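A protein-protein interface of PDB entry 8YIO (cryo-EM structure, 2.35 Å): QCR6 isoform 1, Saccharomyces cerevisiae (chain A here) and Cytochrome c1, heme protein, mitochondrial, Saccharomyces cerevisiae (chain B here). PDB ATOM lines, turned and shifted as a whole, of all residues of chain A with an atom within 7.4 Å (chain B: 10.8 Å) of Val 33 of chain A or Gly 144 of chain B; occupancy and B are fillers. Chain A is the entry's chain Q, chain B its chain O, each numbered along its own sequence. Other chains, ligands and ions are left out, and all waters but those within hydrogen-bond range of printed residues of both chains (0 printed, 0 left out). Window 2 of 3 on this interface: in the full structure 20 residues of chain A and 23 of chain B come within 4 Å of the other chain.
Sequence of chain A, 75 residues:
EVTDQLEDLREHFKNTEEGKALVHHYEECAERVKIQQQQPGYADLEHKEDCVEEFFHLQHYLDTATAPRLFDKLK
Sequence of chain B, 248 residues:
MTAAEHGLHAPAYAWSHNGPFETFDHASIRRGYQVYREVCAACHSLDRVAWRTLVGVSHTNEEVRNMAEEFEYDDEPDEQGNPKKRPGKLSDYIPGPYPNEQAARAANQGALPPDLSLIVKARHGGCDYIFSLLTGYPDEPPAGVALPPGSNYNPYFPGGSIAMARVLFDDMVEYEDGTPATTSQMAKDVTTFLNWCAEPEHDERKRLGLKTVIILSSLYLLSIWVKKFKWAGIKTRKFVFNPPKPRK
O of Asp 50 of chain A sits at hydrogen-bond distance from SG of Cys 29 of chain A, 3.6 Å away. The backbone carbonyl oxygen of Cys 29 of chain A sits at hydrogen-bond distance from the side-chain sulfur of Cys 51 of chain A, 3.7 Å away.
Of chain B, only Gly 144 comes within 4 Å of Val 33 of chain A. Gly 144 of chain B touches two residues of chain A. No residue of chain B comes within 4 Å of Cys 29 of chain A. No residue of chain B comes within 4 Å of Gln 36 of chain A. Asp 50 of chain A touches just these residues of chain B: Ala 143 (3.5 Å), Gly 144 (3.1 Å) and Val 145 (3.6 Å). Of the printed residues of chain A, Val 145 of chain B touches Asp 50 (3.6 Å) and Val 52 (3.7 Å). Printed residues of chain A within 4 Å of Ala 143 of chain B: Tyr 26, Asp 50 and Cys 51. The nearest printed residue of chain A that does not touch Ala 143 of chain B is Ala 30 of chain A (4.1 Å).
Among the printed residues, merely in contact across the chains: Tyr 26 of chain A with Pro 142 of chain B, Tyr 26 of chain A with Ala 143 of chain B, Val 33 of chain A with Gly 144 of chain B, Asp 50 of chain A with Ala 143 of chain B, Asp 50 of chain A with Val 145 of chain B and Val 52 of chain A with Val 145 of chain B.
Printed residues of chain B that touch a printed residue of chain A: Pro 142, Ala 143, Gly 144 and Val 145. Among the printed residues, 8 pairs touch across the chains. Among the printed residues, no Asp or Glu carboxylate lies within 4 Å of a Lys or Arg side-chain nitrogen of the other chain.
O of Ala 143 of chain B sits at hydrogen-bond distance from N of Cys 51 of chain A (3.2 Å). OD1 of Asp 50 of chain A sits close to O of Gly 144 of chain B.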
ATOM      1  N   TYR A  26      17.664  35.147  -5.655  1.00  0.00           N
ATOM      2  CA  TYR A  26      17.830  34.192  -4.566  1.00  0.00           C
ATOM      3  C   TYR A  26      17.304  32.816  -4.955  1.00  0.00           C
ATOM      4  O   TYR A  26      17.891  31.794  -4.581  1.00  0.00           O
ATOM      5  CB  TYR A  26      17.129  34.701  -3.305  1.00  0.00           C
ATOM      6  CG  TYR A  26      17.081  33.684  -2.187  1.00  0.00           C
ATOM      7  CD1 TYR A  26      18.215  33.393  -1.442  1.00  0.00           C
ATOM      8  CD2 TYR A  26      15.902  33.011  -1.882  1.00  0.00           C
ATOM      9  CE1 TYR A  26      18.179  32.461  -0.425  1.00  0.00           C
ATOM     10  CE2 TYR A  26      15.858  32.077  -0.872  1.00  0.00           C
ATOM     11  CZ  TYR A  26      16.998  31.807  -0.145  1.00  0.00           C
ATOM     12  OH  TYR A  26      16.955  30.877   0.865  1.00  0.00           O
ATOM     13  N   GLU A  28      17.170  31.456  -7.959  1.00  0.00           N
ATOM     14  CA  GLU A  28      18.065  30.768  -8.885  1.00  0.00           C
ATOM     15  C   GLU A  28      19.313  30.251  -8.185  1.00  0.00           C
ATOM     16  O   GLU A  28      19.874  29.234  -8.607  1.00  0.00           O
ATOM     17  CB  GLU A  28      18.443  31.683 -10.046  1.00  0.00           C
ATOM     18  CG  GLU A  28      17.250  32.251 -10.778  1.00  0.00           C
ATOM     19  CD  GLU A  28      17.621  33.389 -11.701  1.00  0.00           C
ATOM     20  OE1 GLU A  28      17.729  33.149 -12.921  1.00  0.00           O
ATOM     21  OE2 GLU A  28      17.808  34.520 -11.208  1.00  0.00           O
ATOM     22  N   CYS A  29      19.778  30.911  -7.122  1.00  0.00           N
ATOM     23  CA  CYS A  29      20.904  30.278  -6.402  1.00  0.00           C
ATOM     24  C   CYS A  29      20.349  29.141  -5.536  1.00  0.00           C
ATOM     25  O   CYS A  29      21.097  28.234  -5.309  1.00  0.00           O
ATOM     26  CB  CYS A  29      21.776  31.274  -5.622  1.00  0.00           C
ATOM     27  SG  CYS A  29      22.646  30.616  -4.185  1.00  0.00           S
ATOM     28  N   ALA A  30      19.079  29.185  -5.084  1.00  0.00           N
ATOM     29  CA  ALA A  30      18.562  28.161  -4.184  1.00  0.00           C
ATOM     30  C   ALA A  30      18.361  26.832  -4.894  1.00  0.00           C
ATOM     31  O   ALA A  30      18.496  25.774  -4.271  1.00  0.00           O
ATOM     32  CB  ALA A  30      17.248  28.630  -3.561  1.00  0.00           C
ATOM     33  N   GLU A  31      18.035  26.862  -6.184  1.00  0.00           N
ATOM     34  CA  GLU A  31      17.946  25.618  -6.932  1.00  0.00           C
ATOM     35  C   GLU A  31      19.304  25.125  -7.412  1.00  0.00           C
ATOM     36  O   GLU A  31      19.419  23.956  -7.779  1.00  0.00           O
ATOM     37  CB  GLU A  31      17.004  25.771  -8.127  1.00  0.00           C
ATOM     38  CG  GLU A  31      17.322  26.948  -9.026  1.00  0.00           C
ATOM     39  CD  GLU A  31      16.407  27.017 -10.236  1.00  0.00           C
ATOM     40  OE1 GLU A  31      16.756  26.432 -11.284  1.00  0.00           O
ATOM     41  OE2 GLU A  31      15.335  27.648 -10.135  1.00  0.00           O
ATOM     42  N   ARG A  32      20.336  25.968  -7.399  1.00  0.00           N
ATOM     43  CA  ARG A  32      21.662  25.479  -7.755  1.00  0.00           C
ATOM     44  C   ARG A  32      22.277  24.666  -6.627  1.00  0.00           C
ATOM     45  O   ARG A  32      22.981  23.688  -6.889  1.00  0.00           O
ATOM     46  CB  ARG A  32      22.585  26.634  -8.128  1.00  0.00           C
ATOM     47  CG  ARG A  32      22.325  27.220  -9.498  1.00  0.00           C
ATOM     48  CD  ARG A  32      23.558  27.928 -10.029  1.00  0.00           C
ATOM     49  NE  ARG A  32      23.972  29.051  -9.192  1.00  0.00           N
ATOM     50  CZ  ARG A  32      25.086  29.067  -8.467  1.00  0.00           C
ATOM     51  NH1 ARG A  32      25.390  30.129  -7.732  1.00  0.00           N
ATOM     52  NH2 ARG A  32      25.893  28.015  -8.473  1.00  0.00           N
ATOM     53  N   VAL A  33      22.014  25.046  -5.373  1.00  0.00           N
ATOM     54  CA  VAL A  33      22.499  24.284  -4.225  1.00  0.00           C
ATOM     55  C   VAL A  33      21.793  22.933  -4.135  1.00  0.00           C
ATOM     56  O   VAL A  33      22.353  21.973  -3.589  1.00  0.00           O
ATOM     57  CB  VAL A  33      22.326  25.135  -2.946  1.00  0.00           C
ATOM     58  CG1 VAL A  33      22.987  24.498  -1.728  1.00  0.00           C
ATOM     59  CG2 VAL A  33      22.895  26.521  -3.159  1.00  0.00           C
ATOM     60  N   LYS A  34      20.589  22.829  -4.698  1.00  0.00           N
ATOM     61  CA  LYS A  34      19.841  21.580  -4.792  1.00  0.00           C
ATOM     62  C   LYS A  34      20.567  20.529  -5.625  1.00  0.00           C
ATOM     63  O   LYS A  34      20.875  19.445  -5.122  1.00  0.00           O
ATOM     64  CB  LYS A  34      18.461  21.846  -5.393  1.00  0.00           C
ATOM     65  CG  LYS A  34      17.366  20.931  -4.884  1.00  0.00           C
ATOM     66  CD  LYS A  34      16.074  21.158  -5.651  1.00  0.00           C
ATOM     67  CE  LYS A  34      14.877  20.559  -4.932  1.00  0.00           C
ATOM     68  NZ  LYS A  34      15.118  19.152  -4.506  1.00  0.00           N
ATOM     69  N   ILE A  35      20.830  20.845  -6.898  1.00  0.00           N
ATOM     70  CA  ILE A  35      21.495  19.910  -7.806  1.00  0.00           C
ATOM     71  C   ILE A  35      22.932  19.624  -7.363  1.00  0.00           C
ATOM     72  O   ILE A  35      23.389  18.474  -7.449  1.00  0.00           O
ATOM     73  CB  ILE A  35      21.417  20.444  -9.259  1.00  0.00           C
ATOM     74  CG1 ILE A  35      20.019  20.236  -9.855  1.00  0.00           C
ATOM     75  CG2 ILE A  35      22.421  19.784 -10.187  1.00  0.00           C
ATOM     76  CD1 ILE A  35      19.071  21.399  -9.743  1.00  0.00           C
ATOM     77  N   GLN A  36      23.625  20.632  -6.807  1.00  0.00           N
ATOM     78  CA  GLN A  36      25.074  20.596  -6.584  1.00  0.00           C
ATOM     79  C   GLN A  36      25.522  19.481  -5.649  1.00  0.00           C
ATOM     80  O   GLN A  36      26.553  18.852  -5.910  1.00  0.00           O
ATOM     81  CB  GLN A  36      25.543  21.942  -6.025  1.00  0.00           C
ATOM     82  CG  GLN A  36      27.038  22.087  -5.795  1.00  0.00           C
ATOM     83  CD  GLN A  36      27.359  23.150  -4.759  1.00  0.00           C
ATOM     84  OE1 GLN A  36      26.736  24.211  -4.731  1.00  0.00           O
ATOM     85  NE2 GLN A  36      28.332  22.869  -3.901  1.00  0.00           N
ATOM     86  N   GLN A  37      24.763  19.191  -4.591  1.00  0.00           N
ATOM     87  CA  GLN A  37      25.163  18.096  -3.717  1.00  0.00           C
ATOM     88  C   GLN A  37      24.010  17.174  -3.340  1.00  0.00           C
ATOM     89  O   GLN A  37      23.995  16.650  -2.220  1.00  0.00           O
ATOM     90  CB  GLN A  37      25.823  18.603  -2.433  1.00  0.00           C
ATOM     91  CG  GLN A  37      27.207  19.207  -2.615  1.00  0.00           C
ATOM     92  CD  GLN A  37      27.874  19.465  -1.292  1.00  0.00           C
ATOM     93  OE1 GLN A  37      27.284  19.231  -0.233  1.00  0.00           O
ATOM     94  NE2 GLN A  37      29.117  19.923  -1.336  1.00  0.00           N
ATOM     95  N   GLN A  38      23.043  16.957  -4.232  1.00  0.00           N
ATOM     96  CA  GLN A  38      22.058  15.907  -3.994  1.00  0.00           C
ATOM     97  C   GLN A  38      22.596  14.554  -4.436  1.00  0.00           C
ATOM     98  O   GLN A  38      22.714  13.624  -3.629  1.00  0.00           O
ATOM     99  CB  GLN A  38      20.750  16.220  -4.716  1.00  0.00           C
ATOM    100  CG  GLN A  38      19.650  15.207  -4.447  1.00  0.00           C
ATOM    101  CD  GLN A  38      18.281  15.849  -4.352  1.00  0.00           C
ATOM    102  OE1 GLN A  38      18.025  16.878  -4.971  1.00  0.00           O
ATOM    103  NE2 GLN A  38      17.391  15.240  -3.576  1.00  0.00           N
ATOM    104  N   LYS A  48      31.581  24.254  -0.055  1.00  0.00           N
ATOM    105  CA  LYS A  48      30.294  24.206  -0.729  1.00  0.00           C
ATOM    106  C   LYS A  48      29.596  25.556  -0.635  1.00  0.00           C
ATOM    107  O   LYS A  48      29.895  26.381   0.232  1.00  0.00           O
ATOM    108  CB  LYS A  48      29.418  23.097  -0.143  1.00  0.00           C
ATOM    109  CG  LYS A  48      29.075  23.264   1.324  1.00  0.00           C
ATOM    110  CD  LYS A  48      28.288  22.061   1.794  1.00  0.00           C
ATOM    111  CE  LYS A  48      29.202  20.851   1.913  1.00  0.00           C
ATOM    112  NZ  LYS A  48      28.484  19.648   2.419  1.00  0.00           N
ATOM    113  N   GLU A  49      28.656  25.766  -1.548  1.00  0.00           N
ATOM    114  CA  GLU A  49      28.055  27.070  -1.777  1.00  0.00           C
ATOM    115  C   GLU A  49      26.819  27.272  -0.905  1.00  0.00           C
ATOM    116  O   GLU A  49      26.045  26.342  -0.664  1.00  0.00           O
ATOM    117  CB  GLU A  49      27.693  27.211  -3.259  1.00  0.00           C
ATOM    118  CG  GLU A  49      28.858  27.265  -4.225  1.00  0.00           C
ATOM    119  CD  GLU A  49      28.409  27.332  -5.670  1.00  0.00           C
ATOM    120  OE1 GLU A  49      27.202  27.145  -5.927  1.00  0.00           O
ATOM    121  OE2 GLU A  49      29.262  27.573  -6.550  1.00  0.00           O
ATOM    122  N   ASP A  50      26.648  28.504  -0.427  1.00  0.00           N
ATOM    123  CA  ASP A  50      25.452  28.939   0.279  1.00  0.00           C
ATOM    124  C   ASP A  50      24.738  29.978  -0.575  1.00  0.00           C
ATOM    125  O   ASP A  50      25.195  30.338  -1.662  1.00  0.00           O
ATOM    126  CB  ASP A  50      25.796  29.531   1.651  1.00  0.00           C
ATOM    127  CG  ASP A  50      26.226  28.484   2.646  1.00  0.00           C
ATOM    128  OD1 ASP A  50      25.928  27.295   2.423  1.00  0.00           O
ATOM    129  OD2 ASP A  50      26.859  28.853   3.658  1.00  0.00           O
ATOM    130  N   CYS A  51      23.589  30.441  -0.130  1.00  0.00           N
ATOM    131  CA  CYS A  51      22.908  31.585  -0.719  1.00  0.00           C
ATOM    132  C   CYS A  51      22.801  32.700   0.316  1.00  0.00           C
ATOM    133  O   CYS A  51      21.870  33.392   0.179  1.00  0.00           O
ATOM    134  CB  CYS A  51      21.480  31.243  -1.016  1.00  0.00           C
ATOM    135  SG  CYS A  51      21.225  29.712  -1.945  1.00  0.00           S
ATOM    136  N   VAL A  52      23.773  32.900   1.231  1.00  0.00           N
ATOM    137  CA  VAL A  52      23.706  33.899   2.293  1.00  0.00           C
ATOM    138  C   VAL A  52      23.817  35.306   1.716  1.00  0.00           C
ATOM    139  O   VAL A  52      23.086  36.217   2.124  1.00  0.00           O
ATOM    140  CB  VAL A  52      24.797  33.620   3.345  1.00  0.00           C
ATOM    141  CG1 VAL A  52      24.810  34.685   4.429  1.00  0.00           C
ATOM    142  CG2 VAL A  52      24.592  32.257   3.962  1.00  0.00           C
ATOM    143  N   GLU B 140      12.827  29.587   7.535  1.00  0.00           N
ATOM    144  CA  GLU B 140      13.863  28.590   7.322  1.00  0.00           C
ATOM    145  C   GLU B 140      15.145  29.314   6.945  1.00  0.00           C
ATOM    146  O   GLU B 140      15.087  30.432   6.419  1.00  0.00           O
ATOM    147  CB  GLU B 140      13.459  27.575   6.236  1.00  0.00           C
ATOM    148  CG  GLU B 140      13.436  28.103   4.809  1.00  0.00           C
ATOM    149  CD  GLU B 140      12.094  28.685   4.414  1.00  0.00           C
ATOM    150  OE1 GLU B 140      11.566  29.541   5.149  1.00  0.00           O
ATOM    151  OE2 GLU B 140      11.561  28.276   3.362  1.00  0.00           O
ATOM    152  N   PRO B 141      16.309  28.732   7.232  1.00  0.00           N
ATOM    153  CA  PRO B 141      17.580  29.362   6.838  1.00  0.00           C
ATOM    154  C   PRO B 141      17.770  29.336   5.331  1.00  0.00           C
ATOM    155  O   PRO B 141      17.048  28.619   4.622  1.00  0.00           O
ATOM    156  CB  PRO B 141      18.635  28.496   7.553  1.00  0.00           C
ATOM    157  CG  PRO B 141      17.943  27.234   7.892  1.00  0.00           C
ATOM    158  CD  PRO B 141      16.530  27.611   8.161  1.00  0.00           C
ATOM    159  N   PRO B 142      18.709  30.128   4.796  1.00  0.00           N
ATOM    160  CA  PRO B 142      19.013  30.051   3.362  1.00  0.00           C
ATOM    161  C   PRO B 142      19.585  28.700   2.957  1.00  0.00           C
ATOM    162  O   PRO B 142      20.040  27.909   3.787  1.00  0.00           O
ATOM    163  CB  PRO B 142      20.042  31.167   3.157  1.00  0.00           C
ATOM    164  CG  PRO B 142      19.763  32.128   4.234  1.00  0.00           C
ATOM    165  CD  PRO B 142      19.329  31.316   5.412  1.00  0.00           C
ATOM    166  N   ALA B 143      19.547  28.444   1.651  1.00  0.00           N
ATOM    167  CA  ALA B 143      19.930  27.143   1.119  1.00  0.00           C
ATOM    168  C   ALA B 143      21.431  26.927   1.246  1.00  0.00           C
ATOM    169  O   ALA B 143      22.231  27.748   0.790  1.00  0.00           O
ATOM    170  CB  ALA B 143      19.499  27.026  -0.341  1.00  0.00           C
ATOM    171  N   GLY B 144      21.810  25.819   1.887  1.00  0.00           N
ATOM    172  CA  GLY B 144      23.193  25.457   2.103  1.00  0.00           C
ATOM    173  C   GLY B 144      23.618  25.504   3.557  1.00  0.00           C
ATOM    174  O   GLY B 144      24.504  24.741   3.958  1.00  0.00           O
ATOM    175  N   VAL B 145      23.007  26.381   4.349  1.00  0.00           N
ATOM    176  CA  VAL B 145      23.394  26.568   5.744  1.00  0.00           C
ATOM    177  C   VAL B 145      22.858  25.406   6.569  1.00  0.00           C
ATOM    178  O   VAL B 145      21.647  25.168   6.614  1.00  0.00           O
ATOM    179  CB  VAL B 145      22.879  27.909   6.281  1.00  0.00           C
ATOM    180  CG1 VAL B 145      23.102  28.005   7.785  1.00  0.00           C
ATOM    181  CG2 VAL B 145      23.563  29.049   5.571  1.00  0.00           C
ATOM    182  N   ALA B 146      23.760  24.684   7.226  1.00  0.00           N
ATOM    183  CA  ALA B 146      23.408  23.550   8.069  1.00  0.00           C
ATOM    184  C   ALA B 146      23.669  23.938   9.518  1.00  0.00           C
ATOM    185  O   ALA B 146      24.825  24.009   9.948  1.00  0.00           O
ATOM    186  CB  ALA B 146      24.202  22.306   7.677  1.00  0.00           C
ATOM    187  N   LEU B 147      22.605  24.191  10.259  1.00  0.00           N
ATOM    188  CA  LEU B 147      22.758  24.536  11.663  1.00  0.00           C
ATOM    189  C   LEU B 147      23.001  23.275  12.487  1.00  0.00           C
ATOM    190  O   LEU B 147      22.475  22.209  12.155  1.00  0.00           O
ATOM    191  CB  LEU B 147      21.515  25.253  12.180  1.00  0.00           C
ATOM    192  CG  LEU B 147      21.014  26.459  11.389  1.00  0.00           C
ATOM    193  CD1 LEU B 147      19.575  26.756  11.765  1.00  0.00           C
ATOM    194  CD2 LEU B 147      21.899  27.668  11.641  1.00  0.00           C
ATOM    195  N   PRO B 148      23.805  23.360  13.545  1.00  0.00           N
ATOM    196  CA  PRO B 148      23.885  22.250  14.486  1.00  0.00           C
ATOM    197  C   PRO B 148      22.569  22.092  15.228  1.00  0.00           C
ATOM    198  O   PRO B 148      21.806  23.063  15.378  1.00  0.00           O
ATOM    199  CB  PRO B 148      25.021  22.664  15.431  1.00  0.00           C
ATOM    200  CG  PRO B 148      25.155  24.134  15.266  1.00  0.00           C
ATOM    201  CD  PRO B 148      24.771  24.427  13.856  1.00  0.00           C
ATOM    202  N   TYR B 153      18.507  29.944  13.281  1.00  0.00           N
ATOM    203  CA  TYR B 153      19.085  30.910  12.357  1.00  0.00           C
ATOM    204  C   TYR B 153      18.495  32.295  12.596  1.00  0.00           C
ATOM    205  O   TYR B 153      17.272  32.459  12.633  1.00  0.00           O
ATOM    206  CB  TYR B 153      18.871  30.499  10.898  1.00  0.00           C
ATOM    207  CG  TYR B 153      19.560  31.438   9.929  1.00  0.00           C
ATOM    208  CD1 TYR B 153      20.928  31.353   9.708  1.00  0.00           C
ATOM    209  CD2 TYR B 153      18.847  32.428   9.257  1.00  0.00           C
ATOM    210  CE1 TYR B 153      21.565  32.218   8.843  1.00  0.00           C
ATOM    211  CE2 TYR B 153      19.477  33.300   8.398  1.00  0.00           C
ATOM    212  CZ  TYR B 153      20.834  33.186   8.190  1.00  0.00           C
ATOM    213  OH  TYR B 153      21.466  34.046   7.327  1.00  0.00           O
